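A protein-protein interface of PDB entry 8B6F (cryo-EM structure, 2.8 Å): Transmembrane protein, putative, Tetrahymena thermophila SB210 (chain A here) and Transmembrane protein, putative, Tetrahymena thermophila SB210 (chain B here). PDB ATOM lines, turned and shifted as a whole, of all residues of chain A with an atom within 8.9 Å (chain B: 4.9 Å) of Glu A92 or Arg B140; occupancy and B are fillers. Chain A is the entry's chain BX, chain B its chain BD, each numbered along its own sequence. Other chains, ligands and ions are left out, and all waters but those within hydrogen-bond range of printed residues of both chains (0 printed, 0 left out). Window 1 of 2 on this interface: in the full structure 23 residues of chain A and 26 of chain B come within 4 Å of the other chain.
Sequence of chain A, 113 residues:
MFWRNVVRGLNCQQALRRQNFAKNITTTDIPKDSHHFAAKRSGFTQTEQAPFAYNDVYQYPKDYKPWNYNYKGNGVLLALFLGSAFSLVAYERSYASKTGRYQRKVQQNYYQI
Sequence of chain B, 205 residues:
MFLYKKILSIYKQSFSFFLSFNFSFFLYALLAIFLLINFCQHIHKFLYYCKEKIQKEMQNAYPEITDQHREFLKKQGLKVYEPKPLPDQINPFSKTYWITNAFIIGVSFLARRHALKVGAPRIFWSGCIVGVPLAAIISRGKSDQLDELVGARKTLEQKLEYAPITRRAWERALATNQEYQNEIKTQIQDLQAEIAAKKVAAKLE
The guanidinium group of Arg A104 lies close to the guanidinium group of Arg B140. The guanidinium group (NH2) of Arg A104 lies within salt-bridge range of the side-chain carboxylate (OD2) of Asp B144, at 2.7 Å. The side-chain hydroxyl (OH) of Tyr A91 is in hydrogen-bond range of the side-chain carboxylate (OD2) of Asp B144 (3.4 Å). OE2 of Glu A92 is in salt-bridge range of NH1 of Arg B140, at 2.5 Å.
O of Tyr A95 sits at hydrogen-bond distance from OG1 of Thr A99 (3.0 Å). OE1 of Glu A92 lies within salt-bridge range of NE of Arg A104.
Ser A87 touches Ile B137. Ile B137 touches Leu A88 (CD1 to N, 3.3 Å). Tyr A91 touches Gly B141. Asp B144 touches Tyr A95. NH1 of Arg A104 touches CE1 of Phe B93, 3.4 Å away. Tyr A110 touches Phe B93 (CE2 to CD2, 3.4 Å). CG of Lys B142 touches O of Ile A113 (3.7 Å).
Of the printed residues of chain B, Ser A87 touches Ile B137. Printed residues of chain B within 4 Å of Tyr A91: Gly B141 and Asp B144. Glu A92 touches just one residue of chain B: Arg B140 (2.5 Å). Of the printed residues of chain A, Ile B137 touches Ser A87 and Leu A88. Ile B138 touches none of the printed residues of chain A. No residue of chain A comes within 4 Å of Ser B139. Of chain A, only Glu A92 (2.5 Å) and Arg A104 (3.4 Å) come within 4 Å of Arg B140. Of chain A, only Tyr A91 (3.3 Å) comes within 4 Å of Gly B141. Printed residues of chain A within 4 Å of Lys B142: Ile A113 (3.7 Å). Of the printed residues of chain A, Asp B144 touches Tyr A91 (3.4 Å), Tyr A95 (3.4 Å) and Arg A104 (2.7 Å). The nearest printed residue of chain B that does not touch Glu A92 is Phe B93 (5.3 Å). The nearest printed residue of chain A that does not touch Asp B144 is Tyr A110 (5.3 Å).
Of the 13 printed residues of chain B, 6 touch a printed residue of chain A. Hydrophobic or aromatic side chains of chain B that line the printed part of chain A: Phe B93 and Ile B137. Hydrophobic or aromatic side chains of chain A within 4 Å of the printed part of chain B: Leu A88, Tyr A91, Tyr A95 and Tyr A110.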
ATOM      1  N   ALA A  85       0.452   0.243  15.088  1.00  0.00           N
ATOM      2  CA  ALA A  85       0.062  -0.125  13.731  1.00  0.00           C
ATOM      3  C   ALA A  85      -1.411   0.163  13.485  1.00  0.00           C
ATOM      4  O   ALA A  85      -1.784   0.656  12.414  1.00  0.00           O
ATOM      5  CB  ALA A  85       0.371  -1.599  13.478  1.00  0.00           C
ATOM      6  N   PHE A  86      -2.268  -0.138  14.463  1.00  0.00           N
ATOM      7  CA  PHE A  86      -3.680   0.194  14.323  1.00  0.00           C
ATOM      8  C   PHE A  86      -3.877   1.696  14.195  1.00  0.00           C
ATOM      9  O   PHE A  86      -4.683   2.160  13.382  1.00  0.00           O
ATOM     10  CB  PHE A  86      -4.479  -0.337  15.510  1.00  0.00           C
ATOM     11  CG  PHE A  86      -5.849   0.266  15.620  1.00  0.00           C
ATOM     12  CD1 PHE A  86      -6.886  -0.184  14.822  1.00  0.00           C
ATOM     13  CD2 PHE A  86      -6.098   1.293  16.516  1.00  0.00           C
ATOM     14  CE1 PHE A  86      -8.144   0.376  14.916  1.00  0.00           C
ATOM     15  CE2 PHE A  86      -7.352   1.856  16.615  1.00  0.00           C
ATOM     16  CZ  PHE A  86      -8.378   1.396  15.815  1.00  0.00           C
ATOM     17  N   SER A  87      -3.144   2.474  14.990  1.00  0.00           N
ATOM     18  CA  SER A  87      -3.243   3.923  14.888  1.00  0.00           C
ATOM     19  C   SER A  87      -2.825   4.402  13.505  1.00  0.00           C
ATOM     20  O   SER A  87      -3.447   5.307  12.939  1.00  0.00           O
ATOM     21  CB  SER A  87      -2.390   4.581  15.973  1.00  0.00           C
ATOM     22  OG  SER A  87      -2.605   5.980  16.005  1.00  0.00           O
ATOM     23  N   LEU A  88      -1.765   3.813  12.947  1.00  0.00           N
ATOM     24  CA  LEU A  88      -1.314   4.215  11.619  1.00  0.00           C
ATOM     25  C   LEU A  88      -2.376   3.936  10.565  1.00  0.00           C
ATOM     26  O   LEU A  88      -2.709   4.808   9.756  1.00  0.00           O
ATOM     27  CB  LEU A  88      -0.011   3.491  11.275  1.00  0.00           C
ATOM     28  CG  LEU A  88       0.510   3.658   9.847  1.00  0.00           C
ATOM     29  CD1 LEU A  88       0.676   5.124   9.490  1.00  0.00           C
ATOM     30  CD2 LEU A  88       1.825   2.918   9.685  1.00  0.00           C
ATOM     31  N   VAL A  89      -2.921   2.721  10.559  1.00  0.00           N
ATOM     32  CA  VAL A  89      -3.906   2.367   9.543  1.00  0.00           C
ATOM     33  C   VAL A  89      -5.184   3.169   9.740  1.00  0.00           C
ATOM     34  O   VAL A  89      -5.837   3.569   8.770  1.00  0.00           O
ATOM     35  CB  VAL A  89      -4.174   0.852   9.552  1.00  0.00           C
ATOM     36  CG1 VAL A  89      -4.813   0.415  10.861  1.00  0.00           C
ATOM     37  CG2 VAL A  89      -5.042   0.479   8.377  1.00  0.00           C
ATOM     38  N   ALA A  90      -5.564   3.411  10.994  1.00  0.00           N
ATOM     39  CA  ALA A  90      -6.746   4.221  11.262  1.00  0.00           C
ATOM     40  C   ALA A  90      -6.558   5.643  10.757  1.00  0.00           C
ATOM     41  O   ALA A  90      -7.488   6.238  10.200  1.00  0.00           O
ATOM     42  CB  ALA A  90      -7.056   4.218  12.760  1.00  0.00           C
ATOM     43  N   TYR A  91      -5.365   6.211  10.944  1.00  0.00           N
ATOM     44  CA  TYR A  91      -5.109   7.543  10.411  1.00  0.00           C
ATOM     45  C   TYR A  91      -5.146   7.544   8.889  1.00  0.00           C
ATOM     46  O   TYR A  91      -5.661   8.488   8.280  1.00  0.00           O
ATOM     47  CB  TYR A  91      -3.765   8.077  10.897  1.00  0.00           C
ATOM     48  CG  TYR A  91      -3.467   9.437  10.315  1.00  0.00           C
ATOM     49  CD1 TYR A  91      -4.037  10.580  10.853  1.00  0.00           C
ATOM     50  CD2 TYR A  91      -2.644   9.573   9.205  1.00  0.00           C
ATOM     51  CE1 TYR A  91      -3.785  11.823  10.315  1.00  0.00           C
ATOM     52  CE2 TYR A  91      -2.386  10.814   8.658  1.00  0.00           C
ATOM     53  CZ  TYR A  91      -2.960  11.935   9.219  1.00  0.00           C
ATOM     54  OH  TYR A  91      -2.710  13.175   8.684  1.00  0.00           O
ATOM     55  N   GLU A  92      -4.606   6.502   8.256  1.00  0.00           N
ATOM     56  CA  GLU A  92      -4.686   6.408   6.802  1.00  0.00           C
ATOM     57  C   GLU A  92      -6.137   6.443   6.343  1.00  0.00           C
ATOM     58  O   GLU A  92      -6.496   7.198   5.432  1.00  0.00           O
ATOM     59  CB  GLU A  92      -4.004   5.128   6.323  1.00  0.00           C
ATOM     60  CG  GLU A  92      -2.504   5.096   6.548  1.00  0.00           C
ATOM     61  CD  GLU A  92      -1.756   6.031   5.623  1.00  0.00           C
ATOM     62  OE1 GLU A  92      -2.408   6.713   4.806  1.00  0.00           O
ATOM     63  OE2 GLU A  92      -0.513   6.084   5.712  1.00  0.00           O
ATOM     64  N   ARG A  93      -6.985   5.621   6.958  1.00  0.00           N
ATOM     65  CA  ARG A  93      -8.391   5.583   6.573  1.00  0.00           C
ATOM     66  C   ARG A  93      -9.069   6.918   6.850  1.00  0.00           C
ATOM     67  O   ARG A  93      -9.894   7.383   6.057  1.00  0.00           O
ATOM     68  CB  ARG A  93      -9.105   4.450   7.306  1.00  0.00           C
ATOM     69  CG  ARG A  93     -10.418   4.031   6.670  1.00  0.00           C
ATOM     70  CD  ARG A  93     -10.192   3.302   5.357  1.00  0.00           C
ATOM     71  NE  ARG A  93     -11.432   2.763   4.814  1.00  0.00           N
ATOM     72  CZ  ARG A  93     -12.266   3.429   4.026  1.00  0.00           C
ATOM     73  NH1 ARG A  93     -12.028   4.680   3.665  1.00  0.00           N
ATOM     74  NH2 ARG A  93     -13.364   2.822   3.586  1.00  0.00           N
ATOM     75  N   SER A  94      -8.734   7.548   7.978  1.00  0.00           N
ATOM     76  CA  SER A  94      -9.329   8.837   8.311  1.00  0.00           C
ATOM     77  C   SER A  94      -8.951   9.902   7.291  1.00  0.00           C
ATOM     78  O   SER A  94      -9.796  10.703   6.877  1.00  0.00           O
ATOM     79  CB  SER A  94      -8.899   9.270   9.713  1.00  0.00           C
ATOM     80  OG  SER A  94      -9.361   8.361  10.695  1.00  0.00           O
ATOM     81  N   TYR A  95      -7.684   9.930   6.873  1.00  0.00           N
ATOM     82  CA  TYR A  95      -7.267  10.897   5.864  1.00  0.00           C
ATOM     83  C   TYR A  95      -7.979  10.653   4.542  1.00  0.00           C
ATOM     84  O   TYR A  95      -8.401  11.601   3.873  1.00  0.00           O
ATOM     85  CB  TYR A  95      -5.754  10.843   5.671  1.00  0.00           C
ATOM     86  CG  TYR A  95      -5.268  11.739   4.558  1.00  0.00           C
ATOM     87  CD1 TYR A  95      -5.135  13.106   4.751  1.00  0.00           C
ATOM     88  CD2 TYR A  95      -4.946  11.217   3.314  1.00  0.00           C
ATOM     89  CE1 TYR A  95      -4.694  13.928   3.734  1.00  0.00           C
ATOM     90  CE2 TYR A  95      -4.506  12.030   2.291  1.00  0.00           C
ATOM     91  CZ  TYR A  95      -4.380  13.385   2.509  1.00  0.00           C
ATOM     92  OH  TYR A  95      -3.940  14.201   1.495  1.00  0.00           O
ATOM     93  N   ALA A  96      -8.128   9.389   4.149  1.00  0.00           N
ATOM     94  CA  ALA A  96      -8.865   9.092   2.928  1.00  0.00           C
ATOM     95  C   ALA A  96     -10.301   9.590   3.029  1.00  0.00           C
ATOM     96  O   ALA A  96     -10.833  10.172   2.078  1.00  0.00           O
ATOM     97  CB  ALA A  96      -8.832   7.591   2.648  1.00  0.00           C
ATOM     98  N   SER A  97     -10.947   9.363   4.174  1.00  0.00           N
ATOM     99  CA  SER A  97     -12.320   9.822   4.352  1.00  0.00           C
ATOM    100  C   SER A  97     -12.410  11.343   4.301  1.00  0.00           C
ATOM    101  O   SER A  97     -13.339  11.897   3.702  1.00  0.00           O
ATOM    102  CB  SER A  97     -12.877   9.300   5.675  1.00  0.00           C
ATOM    103  OG  SER A  97     -12.916   7.885   5.682  1.00  0.00           O
ATOM    104  N   LYS A  98     -11.459  12.036   4.932  1.00  0.00           N
ATOM    105  CA  LYS A  98     -11.469  13.495   4.902  1.00  0.00           C
ATOM    106  C   LYS A  98     -11.298  14.019   3.484  1.00  0.00           C
ATOM    107  O   LYS A  98     -11.955  14.990   3.091  1.00  0.00           O
ATOM    108  CB  LYS A  98     -10.371  14.047   5.811  1.00  0.00           C
ATOM    109  CG  LYS A  98     -10.834  14.348   7.224  1.00  0.00           C
ATOM    110  CD  LYS A  98     -11.718  15.582   7.268  1.00  0.00           C
ATOM    111  CE  LYS A  98     -12.228  15.835   8.673  1.00  0.00           C
ATOM    112  NZ  LYS A  98     -13.074  17.057   8.745  1.00  0.00           N
ATOM    113  N   THR A  99     -10.418  13.396   2.704  1.00  0.00           N
ATOM    114  CA  THR A  99     -10.235  13.767   1.308  1.00  0.00           C
ATOM    115  C   THR A  99     -11.354  13.258   0.411  1.00  0.00           C
ATOM    116  O   THR A  99     -11.370  13.589  -0.779  1.00  0.00           O
ATOM    117  CB  THR A  99      -8.895  13.239   0.788  1.00  0.00           C
ATOM    118  OG1 THR A  99      -8.853  11.814   0.918  1.00  0.00           O
ATOM    119  CG2 THR A  99      -7.743  13.848   1.568  1.00  0.00           C
ATOM    120  N   ARG A 101     -12.058  10.039  -0.516  1.00  0.00           N
ATOM    121  CA  ARG A 101     -11.590   8.986  -1.400  1.00  0.00           C
ATOM    122  C   ARG A 101     -11.578   7.668  -0.643  1.00  0.00           C
ATOM    123  O   ARG A 101     -11.440   7.640   0.582  1.00  0.00           O
ATOM    124  CB  ARG A 101     -10.184   9.282  -1.933  1.00  0.00           C
ATOM    125  CG  ARG A 101     -10.042  10.631  -2.610  1.00  0.00           C
ATOM    126  CD  ARG A 101      -8.590  10.905  -2.959  1.00  0.00           C
ATOM    127  NE  ARG A 101      -8.418  12.181  -3.642  1.00  0.00           N
ATOM    128  CZ  ARG A 101      -8.511  12.354  -4.953  1.00  0.00           C
ATOM    129  NH1 ARG A 101      -8.790  11.349  -5.767  1.00  0.00           N
ATOM    130  NH2 ARG A 101      -8.319  13.567  -5.462  1.00  0.00           N
ATOM    131  N   TYR A 102     -11.727   6.568  -1.383  1.00  0.00           N
ATOM    132  CA  TYR A 102     -11.639   5.251  -0.767  1.00  0.00           C
ATOM    133  C   TYR A 102     -10.228   4.928  -0.299  1.00  0.00           C
ATOM    134  O   TYR A 102     -10.054   4.034   0.533  1.00  0.00           O
ATOM    135  CB  TYR A 102     -12.113   4.175  -1.745  1.00  0.00           C
ATOM    136  CG  TYR A 102     -13.595   4.220  -2.033  1.00  0.00           C
ATOM    137  CD1 TYR A 102     -14.518   3.794  -1.087  1.00  0.00           C
ATOM    138  CD2 TYR A 102     -14.069   4.673  -3.255  1.00  0.00           C
ATOM    139  CE1 TYR A 102     -15.874   3.830  -1.347  1.00  0.00           C
ATOM    140  CE2 TYR A 102     -15.422   4.712  -3.525  1.00  0.00           C
ATOM    141  CZ  TYR A 102     -16.320   4.289  -2.568  1.00  0.00           C
ATOM    142  OH  TYR A 102     -17.668   4.325  -2.831  1.00  0.00           O
ATOM    143  N   GLN A 103      -9.221   5.628  -0.815  1.00  0.00           N
ATOM    144  CA  GLN A 103      -7.843   5.389  -0.419  1.00  0.00           C
ATOM    145  C   GLN A 103      -7.030   6.643  -0.699  1.00  0.00           C
ATOM    146  O   GLN A 103      -7.425   7.495  -1.498  1.00  0.00           O
ATOM    147  CB  GLN A 103      -7.254   4.179  -1.155  1.00  0.00           C
ATOM    148  CG  GLN A 103      -5.865   3.782  -0.680  1.00  0.00           C
ATOM    149  CD  GLN A 103      -5.391   2.478  -1.287  1.00  0.00           C
ATOM    150  OE1 GLN A 103      -6.114   1.835  -2.047  1.00  0.00           O
ATOM    151  NE2 GLN A 103      -4.169   2.080  -0.949  1.00  0.00           N
ATOM    152  N   ARG A 104      -5.889   6.747  -0.022  1.00  0.00           N
ATOM    153  CA  ARG A 104      -4.997   7.880  -0.228  1.00  0.00           C
ATOM    154  C   ARG A 104      -4.540   7.943  -1.680  1.00  0.00           C
ATOM    155  O   ARG A 104      -4.244   6.920  -2.303  1.00  0.00           O
ATOM    156  CB  ARG A 104      -3.782   7.768   0.696  1.00  0.00           C
ATOM    157  CG  ARG A 104      -2.696   8.805   0.434  1.00  0.00           C
ATOM    158  CD  ARG A 104      -1.469   8.551   1.288  1.00  0.00           C
ATOM    159  NE  ARG A 104      -1.733   8.766   2.705  1.00  0.00           N
ATOM    160  CZ  ARG A 104      -1.638   9.938   3.318  1.00  0.00           C
ATOM    161  NH1 ARG A 104      -1.296  11.036   2.664  1.00  0.00           N
ATOM    162  NH2 ARG A 104      -1.892  10.011   4.621  1.00  0.00           N
ATOM    163  N   LYS A 105      -4.482   9.160  -2.216  1.00  0.00           N
ATOM    164  CA  LYS A 105      -3.961   9.411  -3.558  1.00  0.00           C
ATOM    165  C   LYS A 105      -2.562   9.995  -3.393  1.00  0.00           C
ATOM    166  O   LYS A 105      -2.384  11.208  -3.279  1.00  0.00           O
ATOM    167  CB  LYS A 105      -4.881  10.344  -4.336  1.00  0.00           C
ATOM    168  CG  LYS A 105      -4.408  10.635  -5.751  1.00  0.00           C
ATOM    169  CD  LYS A 105      -5.393  11.527  -6.491  1.00  0.00           C
ATOM    170  CE  LYS A 105      -4.921  11.825  -7.905  1.00  0.00           C
ATOM    171  NZ  LYS A 105      -3.619  12.550  -7.925  1.00  0.00           N
ATOM    172  N   VAL A 106      -1.559   9.119  -3.375  1.00  0.00           N
ATOM    173  CA  VAL A 106      -0.183   9.562  -3.184  1.00  0.00           C
ATOM    174  C   VAL A 106       0.245  10.407  -4.375  1.00  0.00           C
ATOM    175  O   VAL A 106       0.036  10.030  -5.535  1.00  0.00           O
ATOM    176  CB  VAL A 106       0.751   8.358  -2.982  1.00  0.00           C
ATOM    177  CG1 VAL A 106       0.309   7.537  -1.781  1.00  0.00           C
ATOM    178  CG2 VAL A 106       0.802   7.491  -4.233  1.00  0.00           C
ATOM    179  N   TYR A 110       6.686  15.093  -3.005  1.00  0.00           N
ATOM    180  CA  TYR A 110       6.371  15.709  -1.725  1.00  0.00           C
ATOM    181  C   TYR A 110       7.501  16.653  -1.342  1.00  0.00           C
ATOM    182  O   TYR A 110       8.677  16.290  -1.442  1.00  0.00           O
ATOM    183  CB  TYR A 110       6.170  14.653  -0.638  1.00  0.00           C
ATOM    184  CG  TYR A 110       4.884  13.879  -0.783  1.00  0.00           C
ATOM    185  CD1 TYR A 110       3.707  14.340  -0.212  1.00  0.00           C
ATOM    186  CD2 TYR A 110       4.847  12.690  -1.496  1.00  0.00           C
ATOM    187  CE1 TYR A 110       2.529  13.638  -0.345  1.00  0.00           C
ATOM    188  CE2 TYR A 110       3.675  11.980  -1.634  1.00  0.00           C
ATOM    189  CZ  TYR A 110       2.520  12.459  -1.055  1.00  0.00           C
ATOM    190  OH  TYR A 110       1.349  11.752  -1.191  1.00  0.00           O
ATOM    191  N   ILE A 113       7.601  20.907   4.487  1.00  0.00           N
ATOM    192  CA  ILE A 113       6.512  21.697   5.042  1.00  0.00           C
ATOM    193  C   ILE A 113       6.300  21.337   6.506  1.00  0.00           C
ATOM    194  O   ILE A 113       5.589  20.383   6.822  1.00  0.00           O
ATOM    195  CB  ILE A 113       5.216  21.496   4.241  1.00  0.00           C
ATOM    196  N   PRO B  92       8.181  10.143   3.297  1.00  0.00           N
ATOM    197  CA  PRO B  92       7.503   9.090   4.065  1.00  0.00           C
ATOM    198  C   PRO B  92       6.552   8.229   3.251  1.00  0.00           C
ATOM    199  O   PRO B  92       6.011   7.258   3.795  1.00  0.00           O
ATOM    200  CB  PRO B  92       6.742   9.882   5.136  1.00  0.00           C
ATOM    201  CG  PRO B  92       6.453  11.179   4.489  1.00  0.00           C
ATOM    202  CD  PRO B  92       7.614  11.474   3.577  1.00  0.00           C
ATOM    203  N   PHE B  93       6.326   8.551   1.976  1.00  0.00           N
ATOM    204  CA  PHE B  93       5.471   7.764   1.097  1.00  0.00           C
ATOM    205  C   PHE B  93       6.286   7.021   0.043  1.00  0.00           C
ATOM    206  O   PHE B  93       5.818   6.818  -1.080  1.00  0.00           O
ATOM    207  CB  PHE B  93       4.434   8.658   0.419  1.00  0.00           C
ATOM    208  CG  PHE B  93       3.679   9.542   1.366  1.00  0.00           C
ATOM    209  CD1 PHE B  93       2.561   9.074   2.031  1.00  0.00           C
ATOM    210  CD2 PHE B  93       4.082  10.848   1.580  1.00  0.00           C
ATOM    211  CE1 PHE B  93       1.863   9.890   2.899  1.00  0.00           C
ATOM    212  CE2 PHE B  93       3.388  11.667   2.445  1.00  0.00           C
ATOM    213  CZ  PHE B  93       2.277  11.187   3.105  1.00  0.00           C
ATOM    214  N   TRP B  98       9.910   2.714   3.287  1.00  0.00           N
ATOM    215  CA  TRP B  98       9.281   1.554   3.910  1.00  0.00           C
ATOM    216  C   TRP B  98      10.212   0.350   3.952  1.00  0.00           C
ATOM    217  O   TRP B  98      10.116  -0.467   4.874  1.00  0.00           O
ATOM    218  CB  TRP B  98       7.979   1.218   3.189  1.00  0.00           C
ATOM    219  CG  TRP B  98       6.918   2.204   3.523  1.00  0.00           C
ATOM    220  CD1 TRP B  98       6.357   3.120   2.687  1.00  0.00           C
ATOM    221  CD2 TRP B  98       6.311   2.401   4.804  1.00  0.00           C
ATOM    222  NE1 TRP B  98       5.427   3.870   3.366  1.00  0.00           N
ATOM    223  CE2 TRP B  98       5.379   3.446   4.667  1.00  0.00           C
ATOM    224  CE3 TRP B  98       6.460   1.787   6.053  1.00  0.00           C
ATOM    225  CZ2 TRP B  98       4.597   3.892   5.732  1.00  0.00           C
ATOM    226  CZ3 TRP B  98       5.683   2.231   7.108  1.00  0.00           C
ATOM    227  CH2 TRP B  98       4.762   3.274   6.940  1.00  0.00           C
ATOM    228  N   ALA B 135       6.619   7.085  14.239  1.00  0.00           N
ATOM    229  CA  ALA B 135       7.332   8.042  13.403  1.00  0.00           C
ATOM    230  C   ALA B 135       6.656   8.182  12.048  1.00  0.00           C
ATOM    231  O   ALA B 135       6.534   9.291  11.515  1.00  0.00           O
ATOM    232  CB  ALA B 135       8.789   7.610  13.236  1.00  0.00           C
ATOM    233  N   ALA B 136       6.208   7.064  11.473  1.00  0.00           N
ATOM    234  CA  ALA B 136       5.489   7.126  10.205  1.00  0.00           C
ATOM    235  C   ALA B 136       4.216   7.950  10.337  1.00  0.00           C
ATOM    236  O   ALA B 136       3.895   8.754   9.455  1.00  0.00           O
ATOM    237  CB  ALA B 136       5.164   5.715   9.716  1.00  0.00           C
ATOM    238  N   ILE B 137       3.471   7.755  11.425  1.00  0.00           N
ATOM    239  CA  ILE B 137       2.240   8.515  11.626  1.00  0.00           C
ATOM    240  C   ILE B 137       2.548  10.003  11.705  1.00  0.00           C
ATOM    241  O   ILE B 137       1.885  10.829  11.069  1.00  0.00           O
ATOM    242  CB  ILE B 137       1.519   8.032  12.897  1.00  0.00           C
ATOM    243  CG1 ILE B 137       0.996   6.612  12.701  1.00  0.00           C
ATOM    244  CG2 ILE B 137       0.366   8.969  13.258  1.00  0.00           C
ATOM    245  CD1 ILE B 137       0.523   5.954  13.978  1.00  0.00           C
ATOM    246  N   ILE B 138       3.554  10.367  12.500  1.00  0.00           N
ATOM    247  CA  ILE B 138       3.882  11.777  12.681  1.00  0.00           C
ATOM    248  C   ILE B 138       4.308  12.393  11.356  1.00  0.00           C
ATOM    249  O   ILE B 138       3.877  13.493  10.993  1.00  0.00           O
ATOM    250  CB  ILE B 138       4.969  11.936  13.760  1.00  0.00           C
ATOM    251  CG1 ILE B 138       4.434  11.517  15.134  1.00  0.00           C
ATOM    252  CG2 ILE B 138       5.482  13.371  13.814  1.00  0.00           C
ATOM    253  CD1 ILE B 138       3.190  12.251  15.596  1.00  0.00           C
ATOM    254  N   SER B 139       5.168  11.693  10.615  1.00  0.00           N
ATOM    255  CA  SER B 139       5.656  12.232   9.352  1.00  0.00           C
ATOM    256  C   SER B 139       4.524  12.389   8.345  1.00  0.00           C
ATOM    257  O   SER B 139       4.433  13.413   7.659  1.00  0.00           O
ATOM    258  CB  SER B 139       6.756  11.326   8.799  1.00  0.00           C
ATOM    259  OG  SER B 139       7.270  11.836   7.584  1.00  0.00           O
ATOM    260  N   ARG B 140       3.659  11.379   8.233  1.00  0.00           N
ATOM    261  CA  ARG B 140       2.553  11.454   7.284  1.00  0.00           C
ATOM    262  C   ARG B 140       1.574  12.559   7.658  1.00  0.00           C
ATOM    263  O   ARG B 140       1.077  13.275   6.782  1.00  0.00           O
ATOM    264  CB  ARG B 140       1.840  10.107   7.200  1.00  0.00           C
ATOM    265  CG  ARG B 140       2.645   9.047   6.475  1.00  0.00           C
ATOM    266  CD  ARG B 140       1.989   7.685   6.576  1.00  0.00           C
ATOM    267  NE  ARG B 140       2.538   6.756   5.596  1.00  0.00           N
ATOM    268  CZ  ARG B 140       2.023   6.536   4.393  1.00  0.00           C
ATOM    269  NH1 ARG B 140       0.928   7.153   3.985  1.00  0.00           N
ATOM    270  NH2 ARG B 140       2.625   5.677   3.578  1.00  0.00           N
ATOM    271  N   GLY B 141       1.279  12.707   8.950  1.00  0.00           N
ATOM    272  CA  GLY B 141       0.408  13.788   9.377  1.00  0.00           C
ATOM    273  C   GLY B 141       1.000  15.154   9.092  1.00  0.00           C
ATOM    274  O   GLY B 141       0.305  16.058   8.621  1.00  0.00           O
ATOM    275  N   LYS B 142       2.293  15.321   9.366  1.00  0.00           N
ATOM    276  CA  LYS B 142       2.955  16.587   9.077  1.00  0.00           C
ATOM    277  C   LYS B 142       2.891  16.906   7.590  1.00  0.00           C
ATOM    278  O   LYS B 142       2.639  18.052   7.203  1.00  0.00           O
ATOM    279  CB  LYS B 142       4.404  16.531   9.558  1.00  0.00           C
ATOM    280  CG  LYS B 142       5.160  17.843   9.430  1.00  0.00           C
ATOM    281  CD  LYS B 142       6.654  17.651   9.654  1.00  0.00           C
ATOM    282  CE  LYS B 142       6.954  17.141  11.052  1.00  0.00           C
ATOM    283  NZ  LYS B 142       8.417  17.060  11.301  1.00  0.00           N
ATOM    284  N   SER B 143       3.121  15.903   6.740  1.00  0.00           N
ATOM    285  CA  SER B 143       3.039  16.119   5.299  1.00  0.00           C
ATOM    286  C   SER B 143       1.622  16.480   4.871  1.00  0.00           C
ATOM    287  O   SER B 143       1.428  17.347   4.012  1.00  0.00           O
ATOM    288  CB  SER B 143       3.512  14.869   4.556  1.00  0.00           C
ATOM    289  OG  SER B 143       4.856  14.556   4.877  1.00  0.00           O
ATOM    290  N   ASP B 144       0.618  15.824   5.455  1.00  0.00           N
ATOM    291  CA  ASP B 144      -0.759  16.036   5.022  1.00  0.00           C
ATOM    292  C   ASP B 144      -1.303  17.388   5.470  1.00  0.00           C
ATOM    293  O   ASP B 144      -2.145  17.969   4.779  1.00  0.00           O
ATOM    294  CB  ASP B 144      -1.651  14.913   5.551  1.00  0.00           C
ATOM    295  CG  ASP B 144      -1.318  13.568   4.938  1.00  0.00           C
ATOM    296  OD1 ASP B 144      -0.499  13.528   3.999  1.00  0.00           O
ATOM    297  OD2 ASP B 144      -1.871  12.549   5.397  1.00  0.00           O
